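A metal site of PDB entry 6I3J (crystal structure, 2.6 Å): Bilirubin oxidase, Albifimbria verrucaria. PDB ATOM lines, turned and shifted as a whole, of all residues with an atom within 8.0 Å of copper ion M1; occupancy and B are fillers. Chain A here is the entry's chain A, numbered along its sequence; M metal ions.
Copper ion M1 is bound by a ring nitrogen (NE2) of His 136 (2.0 Å), a ring nitrogen (NE2) of His 403 (2.0 Å) and a ring nitrogen (NE2) of His 456 (2.1 Å).
Copper ion M1 has three donor atoms within binding distance.
A ring nitrogen (ND1) of His 403 lies close to a ring nitrogen (NE2) of His 94 (3.5 Å).
A ring nitrogen (ND1) of His 403 is in hydrogen-bond range of the side-chain carboxylate of Asp 105, 2.7 Å away.
ND1 of His 136 lies close to OE2 of Glu 463, at 3.5 Å.
The backbone NH (N) of His 403 sits at hydrogen-bond distance from the backbone carbonyl oxygen (O) of Met 454 (3.1 Å).
O of His 136 sits close to OG1 of Thr 141 (3.4 Å).
The backbone NH (N) of His 401 sits at hydrogen-bond distance from the backbone carbonyl oxygen (O) of His 456, at 2.9 Å.
A ring nitrogen (ND1) of His 456 lies close to the side-chain carboxylate (OE1) of Glu 463 (3.2 Å).
A ring nitrogen (ND1) of His 401 sits close to a ring nitrogen (NE2) of His 96 (3.4 Å).
His 401 touches copper ion M1 (CD2 to CU, 3.7 Å).
Four residues have an atom within 4 Å of copper ion M1: His 136, His 401, His 403 and His 456.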
ATOM      1  N   HIS A  94     -21.237   2.165 -22.354  1.00  0.00           N
ATOM      2  CA  HIS A  94     -22.359   2.649 -21.604  1.00  0.00           C
ATOM      3  C   HIS A  94     -22.506   4.152 -21.801  1.00  0.00           C
ATOM      4  O   HIS A  94     -21.606   4.916 -21.408  1.00  0.00           O
ATOM      5  CB  HIS A  94     -22.152   2.360 -20.119  1.00  0.00           C
ATOM      6  CG  HIS A  94     -23.205   2.986 -19.273  1.00  0.00           C
ATOM      7  ND1 HIS A  94     -24.547   2.892 -19.582  1.00  0.00           N
ATOM      8  CD2 HIS A  94     -23.112   3.748 -18.159  1.00  0.00           C
ATOM      9  CE1 HIS A  94     -25.239   3.537 -18.687  1.00  0.00           C
ATOM     10  NE2 HIS A  94     -24.394   4.058 -17.796  1.00  0.00           N
ATOM     11  N   HIS A  96     -23.887   6.921 -20.064  1.00  0.00           N
ATOM     12  CA  HIS A  96     -24.217   7.201 -18.651  1.00  0.00           C
ATOM     13  C   HIS A  96     -25.184   8.390 -18.592  1.00  0.00           C
ATOM     14  O   HIS A  96     -24.882   9.503 -19.053  1.00  0.00           O
ATOM     15  CB  HIS A  96     -22.929   7.449 -17.858  1.00  0.00           C
ATOM     16  CG  HIS A  96     -23.102   7.568 -16.374  1.00  0.00           C
ATOM     17  ND1 HIS A  96     -22.350   6.813 -15.491  1.00  0.00           N
ATOM     18  CD2 HIS A  96     -23.894   8.360 -15.615  1.00  0.00           C
ATOM     19  CE1 HIS A  96     -22.690   7.124 -14.251  1.00  0.00           C
ATOM     20  NE2 HIS A  96     -23.643   8.069 -14.305  1.00  0.00           N
ATOM     21  N   ASP A 105     -27.174  -0.441 -23.222  1.00  0.00           N
ATOM     22  CA  ASP A 105     -26.890   0.305 -22.000  1.00  0.00           C
ATOM     23  C   ASP A 105     -25.472   0.026 -21.489  1.00  0.00           C
ATOM     24  O   ASP A 105     -25.054   0.628 -20.536  1.00  0.00           O
ATOM     25  CB  ASP A 105     -27.894  -0.005 -20.884  1.00  0.00           C
ATOM     26  CG  ASP A 105     -27.861   1.028 -19.786  1.00  0.00           C
ATOM     27  OD1 ASP A 105     -27.921   2.218 -20.134  1.00  0.00           O
ATOM     28  OD2 ASP A 105     -27.733   0.634 -18.592  1.00  0.00           O
ATOM     29  N   GLY A 106     -24.764  -0.916 -22.128  1.00  0.00           N
ATOM     30  CA  GLY A 106     -23.343  -1.165 -21.815  1.00  0.00           C
ATOM     31  C   GLY A 106     -23.168  -2.184 -20.704  1.00  0.00           C
ATOM     32  O   GLY A 106     -22.206  -2.119 -19.921  1.00  0.00           O
ATOM     33  N   TRP A 107     -24.122  -3.120 -20.625  1.00  0.00           N
ATOM     34  CA  TRP A 107     -24.042  -4.291 -19.741  1.00  0.00           C
ATOM     35  C   TRP A 107     -22.616  -4.866 -19.806  1.00  0.00           C
ATOM     36  O   TRP A 107     -22.014  -4.940 -20.894  1.00  0.00           O
ATOM     37  CB  TRP A 107     -25.116  -5.305 -20.129  1.00  0.00           C
ATOM     38  CG  TRP A 107     -25.173  -6.565 -19.329  1.00  0.00           C
ATOM     39  CD1 TRP A 107     -24.722  -7.797 -19.717  1.00  0.00           C
ATOM     40  CD2 TRP A 107     -25.766  -6.759 -18.037  1.00  0.00           C
ATOM     41  NE1 TRP A 107     -24.966  -8.725 -18.746  1.00  0.00           N
ATOM     42  CE2 TRP A 107     -25.612  -8.112 -17.698  1.00  0.00           C
ATOM     43  CE3 TRP A 107     -26.396  -5.905 -17.124  1.00  0.00           C
ATOM     44  CZ2 TRP A 107     -26.071  -8.649 -16.493  1.00  0.00           C
ATOM     45  CZ3 TRP A 107     -26.837  -6.437 -15.925  1.00  0.00           C
ATOM     46  CH2 TRP A 107     -26.674  -7.782 -15.614  1.00  0.00           C
ATOM     47  N   ALA A 108     -22.076  -5.216 -18.639  1.00  0.00           N
ATOM     48  CA  ALA A 108     -20.641  -5.484 -18.510  1.00  0.00           C
ATOM     49  C   ALA A 108     -20.244  -6.749 -19.299  1.00  0.00           C
ATOM     50  O   ALA A 108     -19.137  -6.783 -19.825  1.00  0.00           O
ATOM     51  CB  ALA A 108     -20.243  -5.611 -17.057  1.00  0.00           C
ATOM     52  N   HIS A 134     -18.647   5.777 -21.952  1.00  0.00           N
ATOM     53  CA  HIS A 134     -17.404   5.220 -21.459  1.00  0.00           C
ATOM     54  C   HIS A 134     -17.518   3.707 -21.397  1.00  0.00           C
ATOM     55  O   HIS A 134     -18.623   3.158 -21.473  1.00  0.00           O
ATOM     56  CB  HIS A 134     -17.036   5.796 -20.077  1.00  0.00           C
ATOM     57  CG  HIS A 134     -17.976   5.395 -18.989  1.00  0.00           C
ATOM     58  ND1 HIS A 134     -17.996   4.117 -18.456  1.00  0.00           N
ATOM     59  CD2 HIS A 134     -18.921   6.099 -18.322  1.00  0.00           C
ATOM     60  CE1 HIS A 134     -18.923   4.052 -17.516  1.00  0.00           C
ATOM     61  NE2 HIS A 134     -19.498   5.260 -17.415  1.00  0.00           N
ATOM     62  N   ASP A 135     -16.361   3.058 -21.264  1.00  0.00           N
ATOM     63  CA  ASP A 135     -16.276   1.630 -21.285  1.00  0.00           C
ATOM     64  C   ASP A 135     -16.826   1.048 -19.974  1.00  0.00           C
ATOM     65  O   ASP A 135     -16.770   1.693 -18.906  1.00  0.00           O
ATOM     66  CB  ASP A 135     -14.848   1.158 -21.519  1.00  0.00           C
ATOM     67  CG  ASP A 135     -14.808  -0.313 -21.865  1.00  0.00           C
ATOM     68  OD1 ASP A 135     -15.441  -0.673 -22.913  1.00  0.00           O
ATOM     69  OD2 ASP A 135     -14.203  -1.082 -21.057  1.00  0.00           O
ATOM     70  N   HIS A 136     -17.345  -0.176 -20.083  1.00  0.00           N
ATOM     71  CA  HIS A 136     -18.023  -0.807 -18.972  1.00  0.00           C
ATOM     72  C   HIS A 136     -17.821  -2.332 -19.001  1.00  0.00           C
ATOM     73  O   HIS A 136     -18.586  -3.070 -18.354  1.00  0.00           O
ATOM     74  CB  HIS A 136     -19.515  -0.459 -19.038  1.00  0.00           C
ATOM     75  CG  HIS A 136     -20.150  -0.238 -17.709  1.00  0.00           C
ATOM     76  ND1 HIS A 136     -20.140  -1.200 -16.717  1.00  0.00           N
ATOM     77  CD2 HIS A 136     -20.833   0.819 -17.228  1.00  0.00           C
ATOM     78  CE1 HIS A 136     -20.767  -0.725 -15.679  1.00  0.00           C
ATOM     79  NE2 HIS A 136     -21.205   0.500 -15.961  1.00  0.00           N
ATOM     80  N   THR A 141     -12.861  -2.484 -16.798  1.00  0.00           N
ATOM     81  CA  THR A 141     -13.469  -1.158 -16.972  1.00  0.00           C
ATOM     82  C   THR A 141     -12.458  -0.080 -16.580  1.00  0.00           C
ATOM     83  O   THR A 141     -12.320   0.945 -17.251  1.00  0.00           O
ATOM     84  CB  THR A 141     -14.788  -1.046 -16.177  1.00  0.00           C
ATOM     85  OG1 THR A 141     -15.802  -1.795 -16.852  1.00  0.00           O
ATOM     86  CG2 THR A 141     -15.273   0.377 -16.035  1.00  0.00           C
ATOM     87  N   ALA A 274     -17.984   9.850 -11.771  1.00  0.00           N
ATOM     88  CA  ALA A 274     -19.104   9.697 -12.687  1.00  0.00           C
ATOM     89  C   ALA A 274     -20.168  10.765 -12.460  1.00  0.00           C
ATOM     90  O   ALA A 274     -21.147  10.837 -13.199  1.00  0.00           O
ATOM     91  CB  ALA A 274     -19.712   8.316 -12.607  1.00  0.00           C
ATOM     92  N   HIS A 401     -23.907   4.395  -8.509  1.00  0.00           N
ATOM     93  CA  HIS A 401     -24.589   4.721  -9.716  1.00  0.00           C
ATOM     94  C   HIS A 401     -25.678   3.676  -9.935  1.00  0.00           C
ATOM     95  O   HIS A 401     -25.423   2.491  -9.805  1.00  0.00           O
ATOM     96  CB  HIS A 401     -23.570   4.773 -10.863  1.00  0.00           C
ATOM     97  CG  HIS A 401     -24.221   4.939 -12.185  1.00  0.00           C
ATOM     98  ND1 HIS A 401     -25.259   5.833 -12.384  1.00  0.00           N
ATOM     99  CD2 HIS A 401     -23.998   4.325 -13.372  1.00  0.00           C
ATOM    100  CE1 HIS A 401     -25.654   5.780 -13.630  1.00  0.00           C
ATOM    101  NE2 HIS A 401     -24.887   4.863 -14.271  1.00  0.00           N
ATOM    102  N   ILE A 402     -26.886   4.124 -10.256  1.00  0.00           N
ATOM    103  CA  ILE A 402     -27.967   3.232 -10.587  1.00  0.00           C
ATOM    104  C   ILE A 402     -28.359   3.519 -12.033  1.00  0.00           C
ATOM    105  O   ILE A 402     -28.756   4.618 -12.313  1.00  0.00           O
ATOM    106  CB  ILE A 402     -29.153   3.409  -9.621  1.00  0.00           C
ATOM    107  CG1 ILE A 402     -28.730   3.216  -8.162  1.00  0.00           C
ATOM    108  CG2 ILE A 402     -30.283   2.474 -10.000  1.00  0.00           C
ATOM    109  CD1 ILE A 402     -29.822   3.517  -7.167  1.00  0.00           C
ATOM    110  N   HIS A 403     -28.240   2.514 -12.919  1.00  0.00           N
ATOM    111  CA  HIS A 403     -28.613   2.639 -14.334  1.00  0.00           C
ATOM    112  C   HIS A 403     -30.135   2.804 -14.457  1.00  0.00           C
ATOM    113  O   HIS A 403     -30.875   2.552 -13.510  1.00  0.00           O
ATOM    114  CB  HIS A 403     -28.156   1.419 -15.133  1.00  0.00           C
ATOM    115  CG  HIS A 403     -26.667   1.328 -15.324  1.00  0.00           C
ATOM    116  ND1 HIS A 403     -26.097   1.305 -16.597  1.00  0.00           N
ATOM    117  CD2 HIS A 403     -25.656   1.227 -14.439  1.00  0.00           C
ATOM    118  CE1 HIS A 403     -24.785   1.210 -16.465  1.00  0.00           C
ATOM    119  NE2 HIS A 403     -24.487   1.142 -15.138  1.00  0.00           N
ATOM    120  N   TYR A 453     -30.845  -4.245 -15.568  1.00  0.00           N
ATOM    121  CA  TYR A 453     -29.858  -3.146 -15.539  1.00  0.00           C
ATOM    122  C   TYR A 453     -28.892  -3.349 -14.364  1.00  0.00           C
ATOM    123  O   TYR A 453     -29.176  -4.119 -13.450  1.00  0.00           O
ATOM    124  CB  TYR A 453     -30.563  -1.786 -15.414  1.00  0.00           C
ATOM    125  CG  TYR A 453     -31.383  -1.372 -16.616  1.00  0.00           C
ATOM    126  CD1 TYR A 453     -30.811  -0.661 -17.673  1.00  0.00           C
ATOM    127  CD2 TYR A 453     -32.725  -1.676 -16.695  1.00  0.00           C
ATOM    128  CE1 TYR A 453     -31.562  -0.305 -18.774  1.00  0.00           C
ATOM    129  CE2 TYR A 453     -33.489  -1.314 -17.794  1.00  0.00           C
ATOM    130  CZ  TYR A 453     -32.906  -0.630 -18.845  1.00  0.00           C
ATOM    131  OH  TYR A 453     -33.674  -0.269 -19.899  1.00  0.00           O
ATOM    132  N   MET A 454     -27.770  -2.611 -14.405  1.00  0.00           N
ATOM    133  CA  MET A 454     -26.709  -2.630 -13.410  1.00  0.00           C
ATOM    134  C   MET A 454     -26.907  -1.508 -12.370  1.00  0.00           C
ATOM    135  O   MET A 454     -27.612  -0.509 -12.576  1.00  0.00           O
ATOM    136  CB  MET A 454     -25.332  -2.452 -14.074  1.00  0.00           C
ATOM    137  CG  MET A 454     -24.967  -3.589 -15.010  1.00  0.00           C
ATOM    138  SD  MET A 454     -23.282  -3.515 -15.718  1.00  0.00           S
ATOM    139  CE  MET A 454     -23.432  -2.104 -16.813  1.00  0.00           C
ATOM    140  N   PHE A 455     -26.297  -1.729 -11.203  1.00  0.00           N
ATOM    141  CA  PHE A 455     -25.985  -0.687 -10.271  1.00  0.00           C
ATOM    142  C   PHE A 455     -24.729  -1.107  -9.513  1.00  0.00           C
ATOM    143  O   PHE A 455     -24.464  -2.291  -9.353  1.00  0.00           O
ATOM    144  CB  PHE A 455     -27.141  -0.393  -9.333  1.00  0.00           C
ATOM    145  CG  PHE A 455     -27.439  -1.421  -8.268  1.00  0.00           C
ATOM    146  CD1 PHE A 455     -28.159  -2.566  -8.571  1.00  0.00           C
ATOM    147  CD2 PHE A 455     -27.049  -1.209  -6.958  1.00  0.00           C
ATOM    148  CE1 PHE A 455     -28.487  -3.478  -7.572  1.00  0.00           C
ATOM    149  CE2 PHE A 455     -27.370  -2.122  -5.972  1.00  0.00           C
ATOM    150  CZ  PHE A 455     -28.094  -3.258  -6.277  1.00  0.00           C
ATOM    151  N   HIS A 456     -23.954  -0.117  -9.080  1.00  0.00           N
ATOM    152  CA  HIS A 456     -22.638  -0.381  -8.646  1.00  0.00           C
ATOM    153  C   HIS A 456     -21.959   0.868  -8.128  1.00  0.00           C
ATOM    154  O   HIS A 456     -22.400   1.980  -8.368  1.00  0.00           O
ATOM    155  CB  HIS A 456     -21.803  -0.907  -9.798  1.00  0.00           C
ATOM    156  CG  HIS A 456     -21.711   0.021 -10.959  1.00  0.00           C
ATOM    157  ND1 HIS A 456     -20.572   0.756 -11.222  1.00  0.00           N
ATOM    158  CD2 HIS A 456     -22.586   0.297 -11.954  1.00  0.00           C
ATOM    159  CE1 HIS A 456     -20.736   1.421 -12.340  1.00  0.00           C
ATOM    160  NE2 HIS A 456     -21.960   1.147 -12.812  1.00  0.00           N
ATOM    161  N   CYS A 457     -20.868   0.638  -7.405  1.00  0.00           N
ATOM    162  CA  CYS A 457     -19.911   1.655  -7.119  1.00  0.00           C
ATOM    163  C   CYS A 457     -19.171   2.057  -8.405  1.00  0.00           C
ATOM    164  O   CYS A 457     -18.878   1.197  -9.269  1.00  0.00           O
ATOM    165  CB  CYS A 457     -18.920   1.140  -6.080  1.00  0.00           C
ATOM    166  SG  CYS A 457     -17.691   2.389  -5.676  1.00  0.00           S
ATOM    167  N   HIS A 458     -18.894   3.364  -8.536  1.00  0.00           N
ATOM    168  CA  HIS A 458     -18.271   3.901  -9.752  1.00  0.00           C
ATOM    169  C   HIS A 458     -16.794   4.226  -9.508  1.00  0.00           C
ATOM    170  O   HIS A 458     -16.120   4.815 -10.373  1.00  0.00           O
ATOM    171  CB  HIS A 458     -19.082   5.092 -10.305  1.00  0.00           C
ATOM    172  CG  HIS A 458     -19.129   5.142 -11.813  1.00  0.00           C
ATOM    173  ND1 HIS A 458     -18.003   5.395 -12.600  1.00  0.00           N
ATOM    174  CD2 HIS A 458     -20.175   4.982 -12.659  1.00  0.00           C
ATOM    175  CE1 HIS A 458     -18.365   5.383 -13.870  1.00  0.00           C
ATOM    176  NE2 HIS A 458     -19.697   5.131 -13.937  1.00  0.00           N
ATOM    177  N   LEU A 460     -13.806   2.686 -10.223  1.00  0.00           N
ATOM    178  CA  LEU A 460     -13.638   1.669 -11.282  1.00  0.00           C
ATOM    179  C   LEU A 460     -12.842   0.453 -10.759  1.00  0.00           C
ATOM    180  O   LEU A 460     -13.063  -0.679 -11.179  1.00  0.00           O
ATOM    181  CB  LEU A 460     -12.978   2.332 -12.499  1.00  0.00           C
ATOM    182  CG  LEU A 460     -13.815   3.403 -13.221  1.00  0.00           C
ATOM    183  CD1 LEU A 460     -13.220   3.733 -14.596  1.00  0.00           C
ATOM    184  CD2 LEU A 460     -15.271   2.976 -13.379  1.00  0.00           C
ATOM    185  N   GLU A 463     -15.355  -1.376  -8.734  1.00  0.00           N
ATOM    186  CA  GLU A 463     -16.348  -1.845  -9.703  1.00  0.00           C
ATOM    187  C   GLU A 463     -15.855  -3.149 -10.361  1.00  0.00           C
ATOM    188  O   GLU A 463     -16.646  -4.085 -10.557  1.00  0.00           O
ATOM    189  CB  GLU A 463     -16.590  -0.749 -10.747  1.00  0.00           C
ATOM    190  CG  GLU A 463     -17.631  -1.046 -11.841  1.00  0.00           C
ATOM    191  CD  GLU A 463     -17.837   0.056 -12.875  1.00  0.00           C
ATOM    192  OE1 GLU A 463     -17.723   1.291 -12.530  1.00  0.00           O
ATOM    193  OE2 GLU A 463     -18.112  -0.300 -14.065  1.00  0.00           O
ATOM    194  N   MET A 468     -20.712  -4.569  -7.889  1.00  0.00           N
ATOM    195  CA  MET A 468     -21.659  -4.350  -8.943  1.00  0.00           C
ATOM    196  C   MET A 468     -22.716  -5.458  -8.841  1.00  0.00           C
ATOM    197  O   MET A 468     -22.411  -6.589  -8.447  1.00  0.00           O
ATOM    198  CB  MET A 468     -20.922  -4.354 -10.290  1.00  0.00           C
ATOM    199  CG  MET A 468     -21.736  -3.913 -11.482  1.00  0.00           C
ATOM    200  SD  MET A 468     -20.669  -3.307 -12.853  1.00  0.00           S
ATOM    201  CE  MET A 468     -19.415  -4.582 -12.936  1.00  0.00           C
ATOM    202  N   ALA A 469     -23.963  -5.096  -9.131  1.00  0.00           N
ATOM    203  CA  ALA A 469     -25.117  -5.983  -9.006  1.00  0.00           C
ATOM    204  C   ALA A 469     -26.157  -5.595 -10.074  1.00  0.00           C
ATOM    205  O   ALA A 469     -25.895  -4.766 -10.937  1.00  0.00           O
ATOM    206  CB  ALA A 469     -25.677  -5.868  -7.603  1.00  0.00           C
HETATM  207 CU    CU M   1     -22.571   1.264 -14.796  1.00  0.00          CU
HETATM  208 CU    CU M   2     -24.847   4.577 -16.065  1.00  0.00          CU
HETATM  209 CU    CU M   3     -20.646   5.669 -15.807  1.00  0.00          CU
